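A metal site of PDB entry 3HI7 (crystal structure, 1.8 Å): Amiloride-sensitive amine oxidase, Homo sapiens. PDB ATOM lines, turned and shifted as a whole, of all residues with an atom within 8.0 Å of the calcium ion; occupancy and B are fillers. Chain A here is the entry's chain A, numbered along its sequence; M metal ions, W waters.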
ATOM      1  N   LYS A  59      16.375 -17.488  -1.728  1.00  0.00           N
ATOM      2  CA  LYS A  59      16.279 -18.614  -2.655  1.00  0.00           C
ATOM      3  C   LYS A  59      16.888 -18.302  -4.029  1.00  0.00           C
ATOM      4  O   LYS A  59      17.561 -19.126  -4.616  1.00  0.00           O
ATOM      5  CB  LYS A  59      14.802 -19.077  -2.768  1.00  0.00           C
ATOM      6  CG  LYS A  59      14.557 -20.239  -3.714  1.00  0.00           C
ATOM      7  CD  LYS A  59      13.105 -20.744  -3.593  1.00  0.00           C
ATOM      8  CE  LYS A  59      12.754 -21.898  -4.571  1.00  0.00           C
ATOM      9  NZ  LYS A  59      11.250 -22.305  -4.487  1.00  0.00           N
ATOM     10  N   ARG A 325      15.163 -32.069  -8.986  1.00  0.00           N
ATOM     11  CA  ARG A 325      14.553 -31.472  -7.814  1.00  0.00           C
ATOM     12  C   ARG A 325      13.058 -31.792  -7.737  1.00  0.00           C
ATOM     13  O   ARG A 325      12.363 -31.779  -8.765  1.00  0.00           O
ATOM     14  CB  ARG A 325      14.763 -29.967  -7.776  1.00  0.00           C
ATOM     15  CG  ARG A 325      14.301 -29.349  -6.457  1.00  0.00           C
ATOM     16  CD  ARG A 325      14.745 -27.891  -6.297  1.00  0.00           C
ATOM     17  NE  ARG A 325      16.203 -27.758  -6.171  1.00  0.00           N
ATOM     18  CZ  ARG A 325      17.010 -27.164  -7.056  1.00  0.00           C
ATOM     19  NH1 ARG A 325      16.533 -26.589  -8.169  1.00  0.00           N
ATOM     20  NH2 ARG A 325      18.317 -27.129  -6.818  1.00  0.00           N
ATOM     21  N   ILE A 326      12.616 -32.095  -6.520  1.00  0.00           N
ATOM     22  CA  ILE A 326      11.229 -32.305  -6.140  1.00  0.00           C
ATOM     23  C   ILE A 326      10.714 -31.203  -5.207  1.00  0.00           C
ATOM     24  O   ILE A 326       9.599 -30.699  -5.345  1.00  0.00           O
ATOM     25  CB  ILE A 326      11.082 -33.636  -5.360  1.00  0.00           C
ATOM     26  CG1 ILE A 326      11.589 -34.792  -6.200  1.00  0.00           C
ATOM     27  CG2 ILE A 326       9.628 -33.848  -4.906  1.00  0.00           C
ATOM     28  CD1 ILE A 326      11.104 -34.796  -7.626  1.00  0.00           C
ATOM     29  N   ALA A 327      11.520 -30.878  -4.203  1.00  0.00           N
ATOM     30  CA  ALA A 327      11.142 -29.893  -3.204  1.00  0.00           C
ATOM     31  C   ALA A 327      12.322 -29.047  -2.788  1.00  0.00           C
ATOM     32  O   ALA A 327      13.375 -29.567  -2.379  1.00  0.00           O
ATOM     33  CB  ALA A 327      10.520 -30.570  -1.975  1.00  0.00           C
ATOM     34  N   TYR A 328      12.163 -27.732  -2.799  1.00  0.00           N
ATOM     35  CA  TYR A 328      13.196 -26.876  -2.241  1.00  0.00           C
ATOM     36  C   TYR A 328      13.266 -26.914  -0.707  1.00  0.00           C
ATOM     37  O   TYR A 328      14.353 -26.863  -0.126  1.00  0.00           O
ATOM     38  CB  TYR A 328      13.028 -25.442  -2.748  1.00  0.00           C
ATOM     39  CG  TYR A 328      14.133 -24.526  -2.289  1.00  0.00           C
ATOM     40  CD1 TYR A 328      15.391 -24.591  -2.844  1.00  0.00           C
ATOM     41  CD2 TYR A 328      13.912 -23.603  -1.271  1.00  0.00           C
ATOM     42  CE1 TYR A 328      16.415 -23.748  -2.419  1.00  0.00           C
ATOM     43  CE2 TYR A 328      14.933 -22.768  -0.817  1.00  0.00           C
ATOM     44  CZ  TYR A 328      16.184 -22.842  -1.414  1.00  0.00           C
ATOM     45  OH  TYR A 328      17.221 -22.029  -0.985  1.00  0.00           O
ATOM     46  N   GLU A 329      12.106 -26.995  -0.047  1.00  0.00           N
ATOM     47  CA  GLU A 329      11.992 -26.976   1.407  1.00  0.00           C
ATOM     48  C   GLU A 329      10.727 -27.730   1.841  1.00  0.00           C
ATOM     49  O   GLU A 329       9.634 -27.527   1.287  1.00  0.00           O
ATOM     50  CB  GLU A 329      11.949 -25.529   1.945  1.00  0.00           C
ATOM     51  CG  GLU A 329      11.748 -25.404   3.448  1.00  0.00           C
ATOM     52  CD  GLU A 329      11.415 -23.992   3.898  1.00  0.00           C
ATOM     53  OE1 GLU A 329      11.417 -23.070   3.049  1.00  0.00           O
ATOM     54  OE2 GLU A 329      11.100 -23.814   5.097  1.00  0.00           O
ATOM     55  N   ARG A 497       5.255 -26.211   5.894  1.00  0.00           N
ATOM     56  CA  ARG A 497       5.579 -25.522   4.647  1.00  0.00           C
ATOM     57  C   ARG A 497       6.172 -26.545   3.687  1.00  0.00           C
ATOM     58  O   ARG A 497       7.108 -27.264   4.049  1.00  0.00           O
ATOM     59  CB  ARG A 497       6.545 -24.367   4.909  1.00  0.00           C
ATOM     60  CG  ARG A 497       7.033 -23.639   3.641  1.00  0.00           C
ATOM     61  CD  ARG A 497       8.006 -22.577   3.969  1.00  0.00           C
ATOM     62  NE  ARG A 497       8.636 -21.964   2.801  1.00  0.00           N
ATOM     63  CZ  ARG A 497       8.145 -20.921   2.108  1.00  0.00           C
ATOM     64  NH1 ARG A 497       7.015 -20.353   2.443  1.00  0.00           N
ATOM     65  NH2 ARG A 497       8.827 -20.447   1.072  1.00  0.00           N
ATOM     66  N   VAL A 498       5.586 -26.642   2.490  1.00  0.00           N
ATOM     67  CA  VAL A 498       5.970 -27.626   1.477  1.00  0.00           C
ATOM     68  C   VAL A 498       6.241 -26.899   0.159  1.00  0.00           C
ATOM     69  O   VAL A 498       5.367 -26.801  -0.719  1.00  0.00           O
ATOM     70  CB  VAL A 498       4.906 -28.735   1.302  1.00  0.00           C
ATOM     71  CG1 VAL A 498       5.472 -29.912   0.475  1.00  0.00           C
ATOM     72  CG2 VAL A 498       4.399 -29.209   2.682  1.00  0.00           C
ATOM     73  N   ASP A 499       7.441 -26.346   0.060  1.00  0.00           N
ATOM     74  CA  ASP A 499       7.863 -25.632  -1.127  1.00  0.00           C
ATOM     75  C   ASP A 499       8.303 -26.658  -2.174  1.00  0.00           C
ATOM     76  O   ASP A 499       9.500 -26.897  -2.376  1.00  0.00           O
ATOM     77  CB  ASP A 499       8.971 -24.619  -0.797  1.00  0.00           C
ATOM     78  CG  ASP A 499       9.425 -23.834  -2.021  1.00  0.00           C
ATOM     79  OD1 ASP A 499       8.790 -23.926  -3.093  1.00  0.00           O
ATOM     80  OD2 ASP A 499      10.406 -23.105  -1.897  1.00  0.00           O
ATOM     81  N   LEU A 500       7.342 -27.283  -2.836  1.00  0.00           N
ATOM     82  CA  LEU A 500       7.626 -28.155  -3.956  1.00  0.00           C
ATOM     83  C   LEU A 500       8.151 -27.315  -5.120  1.00  0.00           C
ATOM     84  O   LEU A 500       7.608 -26.247  -5.416  1.00  0.00           O
ATOM     85  CB  LEU A 500       6.387 -28.950  -4.390  1.00  0.00           C
ATOM     86  CG  LEU A 500       5.778 -29.860  -3.321  1.00  0.00           C
ATOM     87  CD1 LEU A 500       4.352 -30.281  -3.646  1.00  0.00           C
ATOM     88  CD2 LEU A 500       6.655 -31.099  -3.084  1.00  0.00           C
ATOM     89  N   ASP A 501       9.208 -27.832  -5.767  1.00  0.00           N
ATOM     90  CA  ASP A 501       9.752 -27.290  -6.994  1.00  0.00           C
ATOM     91  C   ASP A 501       9.840 -28.502  -7.918  1.00  0.00           C
ATOM     92  O   ASP A 501      10.915 -29.065  -8.115  1.00  0.00           O
ATOM     93  CB  ASP A 501      11.157 -26.702  -6.788  1.00  0.00           C
ATOM     94  CG  ASP A 501      11.171 -25.309  -6.195  1.00  0.00           C
ATOM     95  OD1 ASP A 501      10.126 -24.726  -5.827  1.00  0.00           O
ATOM     96  OD2 ASP A 501      12.291 -24.773  -6.090  1.00  0.00           O
ATOM     97  N   VAL A 502       8.704 -28.899  -8.482  1.00  0.00           N
ATOM     98  CA  VAL A 502       8.615 -30.162  -9.209  1.00  0.00           C
ATOM     99  C   VAL A 502       9.358 -30.058 -10.544  1.00  0.00           C
ATOM    100  O   VAL A 502       8.915 -29.355 -11.456  1.00  0.00           O
ATOM    101  CB  VAL A 502       7.160 -30.585  -9.409  1.00  0.00           C
ATOM    102  CG1 VAL A 502       7.046 -31.895 -10.187  1.00  0.00           C
ATOM    103  CG2 VAL A 502       6.440 -30.720  -8.060  1.00  0.00           C
ATOM    104  N   GLY A 504      11.937 -28.436 -10.957  1.00  0.00           N
ATOM    105  CA  GLY A 504      12.268 -27.005 -11.112  1.00  0.00           C
ATOM    106  C   GLY A 504      11.246 -26.070 -10.498  1.00  0.00           C
ATOM    107  O   GLY A 504      10.221 -26.510  -9.958  1.00  0.00           O
ATOM    108  N   THR A 505      11.500 -24.760 -10.613  1.00  0.00           N
ATOM    109  CA  THR A 505      10.769 -23.755  -9.909  1.00  0.00           C
ATOM    110  C   THR A 505       9.317 -23.570 -10.416  1.00  0.00           C
ATOM    111  O   THR A 505       8.386 -23.470  -9.638  1.00  0.00           O
ATOM    112  CB  THR A 505      11.594 -22.454 -10.039  1.00  0.00           C
ATOM    113  OG1 THR A 505      12.998 -22.794  -9.973  1.00  0.00           O
ATOM    114  CG2 THR A 505      11.252 -21.501  -8.944  1.00  0.00           C
ATOM    115  N   LYS A 506       9.155 -23.496 -11.741  1.00  0.00           N
ATOM    116  CA  LYS A 506       7.832 -23.162 -12.327  1.00  0.00           C
ATOM    117  C   LYS A 506       6.876 -24.360 -12.399  1.00  0.00           C
ATOM    118  O   LYS A 506       7.079 -25.337 -13.131  1.00  0.00           O
ATOM    119  CB  LYS A 506       7.982 -22.472 -13.670  1.00  0.00           C
ATOM    120  CG  LYS A 506       8.753 -21.125 -13.591  1.00  0.00           C
ATOM    121  CD  LYS A 506       7.876 -19.975 -13.099  1.00  0.00           C
ATOM    122  CE  LYS A 506       8.575 -18.614 -13.227  1.00  0.00           C
ATOM    123  NZ  LYS A 506       8.921 -18.329 -14.662  1.00  0.00           N
ATOM    124  N   ASN A 507       5.811 -24.265 -11.604  1.00  0.00           N
ATOM    125  CA  ASN A 507       4.820 -25.312 -11.499  1.00  0.00           C
ATOM    126  C   ASN A 507       3.400 -24.763 -11.627  1.00  0.00           C
ATOM    127  O   ASN A 507       3.174 -23.538 -11.547  1.00  0.00           O
ATOM    128  CB  ASN A 507       4.907 -25.971 -10.128  1.00  0.00           C
ATOM    129  CG  ASN A 507       6.201 -26.730  -9.884  1.00  0.00           C
ATOM    130  OD1 ASN A 507       6.577 -26.898  -8.711  1.00  0.00           O
ATOM    131  ND2 ASN A 507       6.829 -27.245 -10.932  1.00  0.00           N
ATOM    132  N   PHE A 559       0.910 -31.220  -8.049  1.00  0.00           N
ATOM    133  CA  PHE A 559       1.805 -30.121  -8.390  1.00  0.00           C
ATOM    134  C   PHE A 559       2.584 -30.537  -9.634  1.00  0.00           C
ATOM    135  O   PHE A 559       3.326 -31.526  -9.615  1.00  0.00           O
ATOM    136  CB  PHE A 559       2.661 -29.791  -7.186  1.00  0.00           C
ATOM    137  CG  PHE A 559       1.840 -29.260  -6.051  1.00  0.00           C
ATOM    138  CD1 PHE A 559       1.155 -30.142  -5.219  1.00  0.00           C
ATOM    139  CD2 PHE A 559       1.658 -27.901  -5.871  1.00  0.00           C
ATOM    140  CE1 PHE A 559       0.362 -29.668  -4.197  1.00  0.00           C
ATOM    141  CE2 PHE A 559       0.843 -27.425  -4.857  1.00  0.00           C
ATOM    142  CZ  PHE A 559       0.202 -28.315  -4.018  1.00  0.00           C
ATOM    143  N   THR A 605       0.356 -20.962  -2.117  1.00  0.00           N
ATOM    144  CA  THR A 605       0.736 -19.569  -2.354  1.00  0.00           C
ATOM    145  C   THR A 605       1.852 -19.394  -3.380  1.00  0.00           C
ATOM    146  O   THR A 605       2.636 -20.339  -3.668  1.00  0.00           O
ATOM    147  CB  THR A 605       1.119 -18.831  -1.039  1.00  0.00           C
ATOM    148  OG1 THR A 605       2.335 -19.390  -0.474  1.00  0.00           O
ATOM    149  CG2 THR A 605       0.009 -18.920  -0.007  1.00  0.00           C
ATOM    150  N   LYS A 606       1.911 -18.199  -3.967  1.00  0.00           N
ATOM    151  CA  LYS A 606       3.081 -17.774  -4.740  1.00  0.00           C
ATOM    152  C   LYS A 606       4.257 -17.471  -3.796  1.00  0.00           C
ATOM    153  O   LYS A 606       4.109 -16.742  -2.808  1.00  0.00           O
ATOM    154  CB  LYS A 606       2.728 -16.558  -5.599  1.00  0.00           C
ATOM    155  CG  LYS A 606       3.919 -16.000  -6.373  1.00  0.00           C
ATOM    156  CD  LYS A 606       3.470 -15.014  -7.431  1.00  0.00           C
ATOM    157  CE  LYS A 606       4.632 -14.287  -8.041  1.00  0.00           C
ATOM    158  NZ  LYS A 606       4.177 -13.521  -9.249  1.00  0.00           N
ATOM    159  N   TYR A 607       5.425 -18.054  -4.119  1.00  0.00           N
ATOM    160  CA  TYR A 607       6.640 -17.904  -3.327  1.00  0.00           C
ATOM    161  C   TYR A 607       7.010 -16.428  -3.186  1.00  0.00           C
ATOM    162  O   TYR A 607       7.008 -15.687  -4.175  1.00  0.00           O
ATOM    163  CB  TYR A 607       7.824 -18.649  -3.970  1.00  0.00           C
ATOM    164  CG  TYR A 607       9.092 -18.523  -3.152  1.00  0.00           C
ATOM    165  CD1 TYR A 607       9.901 -17.384  -3.251  1.00  0.00           C
ATOM    166  CD2 TYR A 607       9.471 -19.505  -2.248  1.00  0.00           C
ATOM    167  CE1 TYR A 607      11.037 -17.231  -2.459  1.00  0.00           C
ATOM    168  CE2 TYR A 607      10.598 -19.362  -1.459  1.00  0.00           C
ATOM    169  CZ  TYR A 607      11.378 -18.228  -1.562  1.00  0.00           C
ATOM    170  OH  TYR A 607      12.511 -18.126  -0.773  1.00  0.00           O
ATOM    171  N   GLU A 643       4.208 -20.748 -11.890  1.00  0.00           N
ATOM    172  CA  GLU A 643       4.857 -19.903 -10.894  1.00  0.00           C
ATOM    173  C   GLU A 643       5.574 -20.790  -9.890  1.00  0.00           C
ATOM    174  O   GLU A 643       5.371 -22.003  -9.879  1.00  0.00           O
ATOM    175  CB  GLU A 643       3.848 -19.043 -10.143  1.00  0.00           C
ATOM    176  CG  GLU A 643       3.050 -18.103 -11.008  1.00  0.00           C
ATOM    177  CD  GLU A 643       3.792 -16.823 -11.321  1.00  0.00           C
ATOM    178  OE1 GLU A 643       4.487 -16.309 -10.431  1.00  0.00           O
ATOM    179  OE2 GLU A 643       3.632 -16.317 -12.456  1.00  0.00           O
ATOM    180  N   ASP A 644       6.426 -20.170  -9.072  1.00  0.00           N
ATOM    181  CA  ASP A 644       7.023 -20.834  -7.941  1.00  0.00           C
ATOM    182  C   ASP A 644       5.944 -20.929  -6.852  1.00  0.00           C
ATOM    183  O   ASP A 644       5.565 -19.940  -6.222  1.00  0.00           O
ATOM    184  CB  ASP A 644       8.260 -20.059  -7.471  1.00  0.00           C
ATOM    185  CG  ASP A 644       9.008 -20.782  -6.371  1.00  0.00           C
ATOM    186  OD1 ASP A 644       8.482 -21.804  -5.865  1.00  0.00           O
ATOM    187  OD2 ASP A 644      10.090 -20.303  -6.011  1.00  0.00           O
ATOM    188  N   LEU A 645       5.418 -22.136  -6.674  1.00  0.00           N
ATOM    189  CA  LEU A 645       4.319 -22.374  -5.743  1.00  0.00           C
ATOM    190  C   LEU A 645       4.846 -22.939  -4.422  1.00  0.00           C
ATOM    191  O   LEU A 645       5.884 -23.633  -4.391  1.00  0.00           O
ATOM    192  CB  LEU A 645       3.321 -23.379  -6.348  1.00  0.00           C
ATOM    193  CG  LEU A 645       2.760 -23.017  -7.731  1.00  0.00           C
ATOM    194  CD1 LEU A 645       1.756 -24.114  -8.185  1.00  0.00           C
ATOM    195  CD2 LEU A 645       2.120 -21.633  -7.675  1.00  0.00           C
ATOM    196  N   VAL A 646       4.135 -22.631  -3.340  1.00  0.00           N
ATOM    197  CA  VAL A 646       4.382 -23.190  -2.025  1.00  0.00           C
ATOM    198  C   VAL A 646       3.088 -23.801  -1.541  1.00  0.00           C
ATOM    199  O   VAL A 646       2.045 -23.137  -1.553  1.00  0.00           O
ATOM    200  CB  VAL A 646       4.847 -22.144  -1.018  1.00  0.00           C
ATOM    201  CG1 VAL A 646       5.100 -22.771   0.349  1.00  0.00           C
ATOM    202  CG2 VAL A 646       6.098 -21.435  -1.527  1.00  0.00           C
ATOM    203  N   ALA A 647       3.113 -25.081  -1.192  1.00  0.00           N
ATOM    204  CA  ALA A 647       1.967 -25.745  -0.589  1.00  0.00           C
ATOM    205  C   ALA A 647       2.133 -25.624   0.914  1.00  0.00           C
ATOM    206  O   ALA A 647       3.243 -25.731   1.419  1.00  0.00           O
ATOM    207  CB  ALA A 647       1.878 -27.222  -1.010  1.00  0.00           C
HETATM  208 CA    CA M   1       8.018 -23.998  -5.249  1.00  0.00          CA
HETATM  209  O   HOH W   1       7.138 -24.336  -7.580  1.00  0.00           O
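Lys 59 touches the calcium ion (NZ to CA, 3.7 Å). Of the 25 residues printed, 6 come within 4 Å of the calcium ion.
The side-chain carboxylate of Asp 644 lies within salt-bridge range of the side-chain amino group of Lys 59 (2.8 Å). NZ of Lys 59 lies within salt-bridge range of OD2 of Asp 501 (3.1 Å). The backbone carbonyl oxygen (O) of Asp 499 sits at hydrogen-bond distance from the backbone NH (N) of Tyr 328 (2.8 Å). N of Asp 501 sits at hydrogen-bond distance from O of Ile 326. The backbone NH (N) of Tyr 607 sits at hydrogen-bond distance from the backbone carbonyl oxygen (O) of Asp 644 (2.8 Å). The side-chain carboxylate (OD2) of Asp 499 is in salt-bridge range of the side-chain amino group (NZ) of Lys 59 (2.8 Å). The backbone NH (N) of Asp 499 is in hydrogen-bond range of the backbone carbonyl oxygen (O) of Glu 329 (2.8 Å).
Water W1 lies within hydrogen-bond range of O of Thr 505, OD1 of Asn 507 and N of Leu 645.
The side-chain carboxylate (OD1) of Asp 499 is bound to the calcium ion (2.3 Å). The calcium ion is bound by O of Leu 500, 2.3 Å away. OD1 of Asp 501 binds the calcium ion, 2.3 Å away. OD1 of Asp 644 is bound to the calcium ion (2.3 Å). The backbone carbonyl oxygen (O) of Leu 645 binds the calcium ion. The calcium ion is bound by water W1 (2.5 Å).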
